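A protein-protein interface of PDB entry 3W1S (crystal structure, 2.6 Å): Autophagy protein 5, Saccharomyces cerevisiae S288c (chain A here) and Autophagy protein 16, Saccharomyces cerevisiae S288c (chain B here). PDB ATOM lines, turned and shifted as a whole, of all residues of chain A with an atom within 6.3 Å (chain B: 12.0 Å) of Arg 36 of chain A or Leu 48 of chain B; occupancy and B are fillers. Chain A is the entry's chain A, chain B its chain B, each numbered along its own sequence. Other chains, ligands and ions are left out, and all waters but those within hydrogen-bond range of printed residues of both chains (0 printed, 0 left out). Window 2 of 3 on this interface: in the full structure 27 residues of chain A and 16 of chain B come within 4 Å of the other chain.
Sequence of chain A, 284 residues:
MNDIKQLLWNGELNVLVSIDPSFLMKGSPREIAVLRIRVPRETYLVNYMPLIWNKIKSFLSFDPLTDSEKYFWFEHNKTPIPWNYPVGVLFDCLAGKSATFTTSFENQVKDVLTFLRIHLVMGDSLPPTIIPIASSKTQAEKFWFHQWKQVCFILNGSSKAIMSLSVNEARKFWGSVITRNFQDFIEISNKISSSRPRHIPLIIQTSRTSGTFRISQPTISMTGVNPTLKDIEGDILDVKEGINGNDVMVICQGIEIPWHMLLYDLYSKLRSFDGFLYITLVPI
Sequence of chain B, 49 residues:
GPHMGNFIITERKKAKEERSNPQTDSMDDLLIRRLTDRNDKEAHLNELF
The side-chain amide nitrogen of Asn 14 of chain A sits at hydrogen-bond distance from the backbone carbonyl oxygen of His 44 of chain B. The backbone carbonyl oxygen of Leu 48 of chain B lies within hydrogen-bond range of the guanidinium group of Arg 36 of chain A (2.9 Å). The backbone carbonyl oxygen of Glu 42 of chain B lies within hydrogen-bond range of the guanidinium group of Arg 38 of chain A (3.0 Å).
The side-chain amide oxygen (OD1) of Asn 14 of chain A sits at hydrogen-bond distance from the guanidinium group (NH1) of Arg 38 of chain A. The backbone NH (N) of Val 15 of chain A lies within hydrogen-bond range of the backbone carbonyl oxygen (O) of Ile 37 of chain A. The backbone carbonyl oxygen (O) of Ala 43 of chain B is in hydrogen-bond range of the side-chain amide nitrogen (ND2) of Asn 46 of chain B, at 2.5 Å. OE1 of Glu 47 of chain B sits close to OD1 of Asn 46 of chain B.
Glu 42 of chain B touches Asn 14 of chain A (O to ND2, 3.8 Å). CA of Asn 46 of chain B touches OD1 of Asn 14 of chain A, 3.6 Å away. Phe 49 of chain B touches Asn 14 of chain A. Val 15 of chain A touches Phe 49 of chain B. N of Leu 16 of chain A touches CE1 of Phe 49 of chain B, 3.9 Å away. O of Arg 36 of chain A touches O of Phe 49 of chain B (3.6 Å). Ile 37 of chain A touches Phe 49 of chain B (CA to O, 3.8 Å). Arg 38 of chain A touches Ala 43 of chain B. Phe 49 of chain B touches Arg 38 of chain A. Leu 113 of chain A touches Leu 45 of chain B (CD1 to CB, 3.4 Å).
Of the printed residues of chain B, Asn 14 of chain A touches Glu 42, His 44, Asn 46 and Phe 49. Of chain B, only Phe 49 comes within 4 Å of Leu 16 of chain A. No residue of chain B comes within 4 Å of Val 17 of chain A. No residue of chain B comes within 4 Å of Leu 35 of chain A. Arg 36 of chain A touches just these residues of chain B: Leu 48 (2.9 Å) and Phe 49 (3.6 Å). Ile 37 of chain A touches just one residue of chain B: Phe 49 (3.8 Å). Of the printed residues of chain B, Leu 113 of chain A touches Leu 45. Printed residues of chain A within 4 Å of Ala 43 of chain B: Arg 38. Leu 48 of chain B touches just one residue of chain A: Arg 36. Printed residues of chain A within 4 Å of Phe 49 of chain B: Asn 14 (3.4 Å), Val 15 (3.5 Å), Leu 16 (3.9 Å), Arg 36 (3.6 Å), Ile 37 (3.8 Å) and Arg 38 (3.8 Å). The nearest residue of chain B that does not touch Arg 36 of chain A is Glu 47 of chain B (5.7 Å). The nearest residue of chain A that does not touch Leu 48 of chain B is Leu 113 of chain A (4.5 Å).
Of the 10 printed residues of chain B, 7 touch a printed residue of chain A. Hydrophobic or aromatic side chains of chain A that line the printed part of chain B: Leu 113. Along chain A the printed residues that touch a printed residue of chain B span positions 14 to 113. Among the printed residues, no Asp or Glu carboxylate lies within 4 Å of a Lys or Arg side-chain nitrogen of the other chain.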
ATOM      1  N   ASN A  14      -8.285 -22.791  -0.881  1.00  0.00           N
ATOM      2  CA  ASN A  14      -9.578 -22.496  -1.504  1.00  0.00           C
ATOM      3  C   ASN A  14     -10.595 -22.823  -0.407  1.00  0.00           C
ATOM      4  O   ASN A  14     -10.587 -23.933   0.129  1.00  0.00           O
ATOM      5  CB  ASN A  14      -9.845 -23.412  -2.711  1.00  0.00           C
ATOM      6  CG  ASN A  14      -8.877 -23.181  -3.868  1.00  0.00           C
ATOM      7  OD1 ASN A  14      -8.468 -22.052  -4.152  1.00  0.00           O
ATOM      8  ND2 ASN A  14      -8.532 -24.258  -4.560  1.00  0.00           N
ATOM      9  N   VAL A  15     -11.466 -21.886  -0.057  1.00  0.00           N
ATOM     10  CA  VAL A  15     -12.432 -22.188   0.988  1.00  0.00           C
ATOM     11  C   VAL A  15     -13.851 -22.036   0.500  1.00  0.00           C
ATOM     12  O   VAL A  15     -14.219 -21.015  -0.074  1.00  0.00           O
ATOM     13  CB  VAL A  15     -12.213 -21.300   2.244  1.00  0.00           C
ATOM     14  CG1 VAL A  15     -13.258 -21.624   3.328  1.00  0.00           C
ATOM     15  CG2 VAL A  15     -10.806 -21.528   2.787  1.00  0.00           C
ATOM     16  N   LEU A  16     -14.643 -23.075   0.717  1.00  0.00           N
ATOM     17  CA  LEU A  16     -16.027 -23.055   0.305  1.00  0.00           C
ATOM     18  C   LEU A  16     -16.898 -22.755   1.501  1.00  0.00           C
ATOM     19  O   LEU A  16     -17.132 -23.613   2.356  1.00  0.00           O
ATOM     20  CB  LEU A  16     -16.433 -24.397  -0.316  1.00  0.00           C
ATOM     21  CG  LEU A  16     -17.872 -24.506  -0.861  1.00  0.00           C
ATOM     22  CD1 LEU A  16     -18.136 -23.411  -1.874  1.00  0.00           C
ATOM     23  CD2 LEU A  16     -18.094 -25.866  -1.488  1.00  0.00           C
ATOM     24  N   VAL A  17     -17.363 -21.522   1.606  1.00  0.00           N
ATOM     25  CA  VAL A  17     -18.214 -21.226   2.743  1.00  0.00           C
ATOM     26  C   VAL A  17     -19.710 -21.387   2.393  1.00  0.00           C
ATOM     27  O   VAL A  17     -20.230 -20.737   1.462  1.00  0.00           O
ATOM     28  CB  VAL A  17     -17.970 -19.792   3.254  1.00  0.00           C
ATOM     29  CG1 VAL A  17     -18.517 -19.621   4.664  1.00  0.00           C
ATOM     30  CG2 VAL A  17     -16.436 -19.480   3.289  1.00  0.00           C
ATOM     31  N   VAL A  34     -23.701 -19.414  -0.661  1.00  0.00           N
ATOM     32  CA  VAL A  34     -22.371 -20.006  -0.825  1.00  0.00           C
ATOM     33  C   VAL A  34     -21.237 -19.055  -1.215  1.00  0.00           C
ATOM     34  O   VAL A  34     -21.254 -18.458  -2.294  1.00  0.00           O
ATOM     35  CB  VAL A  34     -22.414 -21.179  -1.832  1.00  0.00           C
ATOM     36  CG1 VAL A  34     -21.057 -21.854  -1.896  1.00  0.00           C
ATOM     37  CG2 VAL A  34     -23.459 -22.186  -1.372  1.00  0.00           C
ATOM     38  N   LEU A  35     -20.240 -18.941  -0.332  1.00  0.00           N
ATOM     39  CA  LEU A  35     -19.069 -18.094  -0.568  1.00  0.00           C
ATOM     40  C   LEU A  35     -17.864 -18.900  -0.983  1.00  0.00           C
ATOM     41  O   LEU A  35     -17.612 -19.977  -0.463  1.00  0.00           O
ATOM     42  CB  LEU A  35     -18.680 -17.287   0.673  1.00  0.00           C
ATOM     43  CG  LEU A  35     -19.527 -16.082   1.065  1.00  0.00           C
ATOM     44  CD1 LEU A  35     -20.855 -16.558   1.646  1.00  0.00           C
ATOM     45  CD2 LEU A  35     -18.755 -15.235   2.071  1.00  0.00           C
ATOM     46  N   ARG A  36     -17.106 -18.348  -1.915  1.00  0.00           N
ATOM     47  CA  ARG A  36     -15.919 -19.004  -2.417  1.00  0.00           C
ATOM     48  C   ARG A  36     -14.802 -18.010  -2.180  1.00  0.00           C
ATOM     49  O   ARG A  36     -14.833 -16.905  -2.718  1.00  0.00           O
ATOM     50  CB  ARG A  36     -16.080 -19.299  -3.908  1.00  0.00           C
ATOM     51  CG  ARG A  36     -17.437 -19.906  -4.260  1.00  0.00           C
ATOM     52  CD  ARG A  36     -17.496 -20.280  -5.723  1.00  0.00           C
ATOM     53  NE  ARG A  36     -16.984 -19.202  -6.562  1.00  0.00           N
ATOM     54  CZ  ARG A  36     -17.671 -18.113  -6.873  1.00  0.00           C
ATOM     55  NH1 ARG A  36     -18.910 -17.972  -6.415  1.00  0.00           N
ATOM     56  NH2 ARG A  36     -17.118 -17.164  -7.622  1.00  0.00           N
ATOM     57  N   ILE A  37     -13.828 -18.387  -1.360  1.00  0.00           N
ATOM     58  CA  ILE A  37     -12.735 -17.476  -1.061  1.00  0.00           C
ATOM     59  C   ILE A  37     -11.363 -18.105  -0.955  1.00  0.00           C
ATOM     60  O   ILE A  37     -11.218 -19.322  -0.873  1.00  0.00           O
ATOM     61  CB  ILE A  37     -13.007 -16.682   0.249  1.00  0.00           C
ATOM     62  CG1 ILE A  37     -13.704 -17.573   1.278  1.00  0.00           C
ATOM     63  CG2 ILE A  37     -13.855 -15.464  -0.050  1.00  0.00           C
ATOM     64  CD1 ILE A  37     -14.080 -16.856   2.563  1.00  0.00           C
ATOM     65  N   ARG A  38     -10.362 -17.236  -0.976  1.00  0.00           N
ATOM     66  CA  ARG A  38      -8.967 -17.613  -0.860  1.00  0.00           C
ATOM     67  C   ARG A  38      -8.534 -17.145   0.523  1.00  0.00           C
ATOM     68  O   ARG A  38      -8.325 -15.953   0.741  1.00  0.00           O
ATOM     69  CB  ARG A  38      -8.139 -16.909  -1.942  1.00  0.00           C
ATOM     70  CG  ARG A  38      -8.332 -17.484  -3.347  1.00  0.00           C
ATOM     71  CD  ARG A  38      -7.745 -18.900  -3.449  1.00  0.00           C
ATOM     72  NE  ARG A  38      -6.284 -18.893  -3.366  1.00  0.00           N
ATOM     73  CZ  ARG A  38      -5.526 -19.983  -3.312  1.00  0.00           C
ATOM     74  NH1 ARG A  38      -6.081 -21.187  -3.325  1.00  0.00           N
ATOM     75  NH2 ARG A  38      -4.208 -19.867  -3.258  1.00  0.00           N
ATOM     76  N   LYS A  55     -21.659 -10.031   2.502  1.00  0.00           N
ATOM     77  CA  LYS A  55     -22.329 -10.724   1.411  1.00  0.00           C
ATOM     78  C   LYS A  55     -23.728 -11.285   1.697  1.00  0.00           C
ATOM     79  O   LYS A  55     -24.504 -11.479   0.765  1.00  0.00           O
ATOM     80  CB  LYS A  55     -21.447 -11.851   0.862  1.00  0.00           C
ATOM     81  CG  LYS A  55     -22.125 -12.633  -0.254  1.00  0.00           C
ATOM     82  CD  LYS A  55     -21.160 -13.499  -1.048  1.00  0.00           C
ATOM     83  CE  LYS A  55     -21.846 -14.078  -2.294  1.00  0.00           C
ATOM     84  NZ  LYS A  55     -20.912 -14.877  -3.143  1.00  0.00           N
ATOM     85  N   LEU A 113      -9.140 -31.417  -6.868  1.00  0.00           N
ATOM     86  CA  LEU A 113      -9.306 -30.061  -6.364  1.00  0.00           C
ATOM     87  C   LEU A 113      -9.098 -30.062  -4.853  1.00  0.00           C
ATOM     88  O   LEU A 113      -9.741 -30.818  -4.123  1.00  0.00           O
ATOM     89  CB  LEU A 113     -10.706 -29.534  -6.691  1.00  0.00           C
ATOM     90  CG  LEU A 113     -11.068 -28.161  -6.119  1.00  0.00           C
ATOM     91  CD1 LEU A 113     -10.375 -27.079  -6.913  1.00  0.00           C
ATOM     92  CD2 LEU A 113     -12.570 -27.968  -6.160  1.00  0.00           C
ATOM     93  N   ASP B  40       1.557 -24.343  -4.783  1.00  0.00           N
ATOM     94  CA  ASP B  40       1.056 -24.596  -6.130  1.00  0.00           C
ATOM     95  C   ASP B  40      -0.098 -25.608  -6.145  1.00  0.00           C
ATOM     96  O   ASP B  40      -1.092 -25.405  -6.845  1.00  0.00           O
ATOM     97  CB  ASP B  40       2.191 -25.091  -7.029  1.00  0.00           C
ATOM     98  CG  ASP B  40       3.123 -23.974  -7.461  1.00  0.00           C
ATOM     99  OD1 ASP B  40       4.209 -24.282  -8.006  1.00  0.00           O
ATOM    100  OD2 ASP B  40       2.770 -22.788  -7.263  1.00  0.00           O
ATOM    101  N   LYS B  41       0.020 -26.693  -5.386  1.00  0.00           N
ATOM    102  CA  LYS B  41      -1.053 -27.676  -5.360  1.00  0.00           C
ATOM    103  C   LYS B  41      -2.299 -27.054  -4.726  1.00  0.00           C
ATOM    104  O   LYS B  41      -3.430 -27.345  -5.126  1.00  0.00           O
ATOM    105  CB  LYS B  41      -0.625 -28.920  -4.579  1.00  0.00           C
ATOM    106  N   GLU B  42      -2.087 -26.182  -3.748  1.00  0.00           N
ATOM    107  CA  GLU B  42      -3.194 -25.539  -3.056  1.00  0.00           C
ATOM    108  C   GLU B  42      -3.768 -24.350  -3.823  1.00  0.00           C
ATOM    109  O   GLU B  42      -4.891 -23.913  -3.552  1.00  0.00           O
ATOM    110  CB  GLU B  42      -2.755 -25.129  -1.641  1.00  0.00           C
ATOM    111  CG  GLU B  42      -2.637 -26.334  -0.702  1.00  0.00           C
ATOM    112  CD  GLU B  42      -2.042 -26.016   0.669  1.00  0.00           C
ATOM    113  OE1 GLU B  42      -1.962 -26.954   1.492  1.00  0.00           O
ATOM    114  OE2 GLU B  42      -1.657 -24.852   0.930  1.00  0.00           O
ATOM    115  N   ALA B  43      -3.005 -23.839  -4.785  1.00  0.00           N
ATOM    116  CA  ALA B  43      -3.464 -22.712  -5.594  1.00  0.00           C
ATOM    117  C   ALA B  43      -4.163 -23.217  -6.862  1.00  0.00           C
ATOM    118  O   ALA B  43      -4.844 -22.461  -7.555  1.00  0.00           O
ATOM    119  CB  ALA B  43      -2.297 -21.822  -5.963  1.00  0.00           C
ATOM    120  N   HIS B  44      -4.001 -24.504  -7.154  1.00  0.00           N
ATOM    121  CA  HIS B  44      -4.614 -25.092  -8.325  1.00  0.00           C
ATOM    122  C   HIS B  44      -6.120 -24.830  -8.349  1.00  0.00           C
ATOM    123  O   HIS B  44      -6.802 -24.975  -7.335  1.00  0.00           O
ATOM    124  CB  HIS B  44      -4.342 -26.598  -8.358  1.00  0.00           C
ATOM    125  CG  HIS B  44      -4.915 -27.283  -9.561  1.00  0.00           C
ATOM    126  ND1 HIS B  44      -4.686 -26.838 -10.847  1.00  0.00           N
ATOM    127  CD2 HIS B  44      -5.743 -28.349  -9.672  1.00  0.00           C
ATOM    128  CE1 HIS B  44      -5.354 -27.597 -11.696  1.00  0.00           C
ATOM    129  NE2 HIS B  44      -6.004 -28.521 -11.009  1.00  0.00           N
ATOM    130  N   LEU B  45      -6.629 -24.442  -9.514  1.00  0.00           N
ATOM    131  CA  LEU B  45      -8.052 -24.153  -9.681  1.00  0.00           C
ATOM    132  C   LEU B  45      -8.550 -23.036  -8.763  1.00  0.00           C
ATOM    133  O   LEU B  45      -9.724 -23.004  -8.384  1.00  0.00           O
ATOM    134  CB  LEU B  45      -8.881 -25.426  -9.461  1.00  0.00           C
ATOM    135  CG  LEU B  45      -8.823 -26.438 -10.609  1.00  0.00           C
ATOM    136  CD1 LEU B  45      -9.717 -27.625 -10.304  1.00  0.00           C
ATOM    137  CD2 LEU B  45      -9.275 -25.754 -11.889  1.00  0.00           C
ATOM    138  N   ASN B  46      -7.654 -22.115  -8.420  1.00  0.00           N
ATOM    139  CA  ASN B  46      -8.005 -21.000  -7.558  1.00  0.00           C
ATOM    140  C   ASN B  46      -8.939 -20.049  -8.307  1.00  0.00           C
ATOM    141  O   ASN B  46      -9.519 -19.137  -7.720  1.00  0.00           O
ATOM    142  CB  ASN B  46      -6.733 -20.276  -7.094  1.00  0.00           C
ATOM    143  CG  ASN B  46      -5.999 -19.586  -8.229  1.00  0.00           C
ATOM    144  OD1 ASN B  46      -6.440 -18.554  -8.733  1.00  0.00           O
ATOM    145  ND2 ASN B  46      -4.872 -20.155  -8.639  1.00  0.00           N
ATOM    146  N   GLU B  47      -9.094 -20.283  -9.607  1.00  0.00           N
ATOM    147  CA  GLU B  47      -9.961 -19.461 -10.450  1.00  0.00           C
ATOM    148  C   GLU B  47     -11.420 -19.652 -10.033  1.00  0.00           C
ATOM    149  O   GLU B  47     -12.249 -18.765 -10.223  1.00  0.00           O
ATOM    150  CB  GLU B  47      -9.801 -19.846 -11.933  1.00  0.00           C
ATOM    151  CG  GLU B  47      -8.385 -19.712 -12.498  1.00  0.00           C
ATOM    152  CD  GLU B  47      -7.437 -20.809 -12.034  1.00  0.00           C
ATOM    153  OE1 GLU B  47      -7.211 -20.941 -10.817  1.00  0.00           O
ATOM    154  OE2 GLU B  47      -6.902 -21.548 -12.885  1.00  0.00           O
ATOM    155  N   LEU B  48     -11.719 -20.814  -9.463  1.00  0.00           N
ATOM    156  CA  LEU B  48     -13.070 -21.139  -9.022  1.00  0.00           C
ATOM    157  C   LEU B  48     -13.379 -20.492  -7.688  1.00  0.00           C
ATOM    158  O   LEU B  48     -14.514 -20.512  -7.224  1.00  0.00           O
ATOM    159  CB  LEU B  48     -13.231 -22.653  -8.880  1.00  0.00           C
ATOM    160  CG  LEU B  48     -12.842 -23.515 -10.081  1.00  0.00           C
ATOM    161  CD1 LEU B  48     -13.130 -24.959  -9.752  1.00  0.00           C
ATOM    162  CD2 LEU B  48     -13.609 -23.076 -11.324  1.00  0.00           C
ATOM    163  N   PHE B  49     -12.358 -19.931  -7.059  1.00  0.00           N
ATOM    164  CA  PHE B  49     -12.544 -19.297  -5.765  1.00  0.00           C
ATOM    165  C   PHE B  49     -12.104 -17.842  -5.828  1.00  0.00           C
ATOM    166  O   PHE B  49     -11.845 -17.288  -4.739  1.00  0.00           O
ATOM    167  CB  PHE B  49     -11.753 -20.062  -4.691  1.00  0.00           C
ATOM    168  CG  PHE B  49     -12.285 -21.450  -4.412  1.00  0.00           C
ATOM    169  CD1 PHE B  49     -13.155 -21.679  -3.346  1.00  0.00           C
ATOM    170  CD2 PHE B  49     -11.938 -22.526  -5.235  1.00  0.00           C
ATOM    171  CE1 PHE B  49     -13.676 -22.959  -3.100  1.00  0.00           C
ATOM    172  CE2 PHE B  49     -12.454 -23.812  -5.002  1.00  0.00           C
ATOM    173  CZ  PHE B  49     -13.322 -24.028  -3.934  1.00  0.00           C
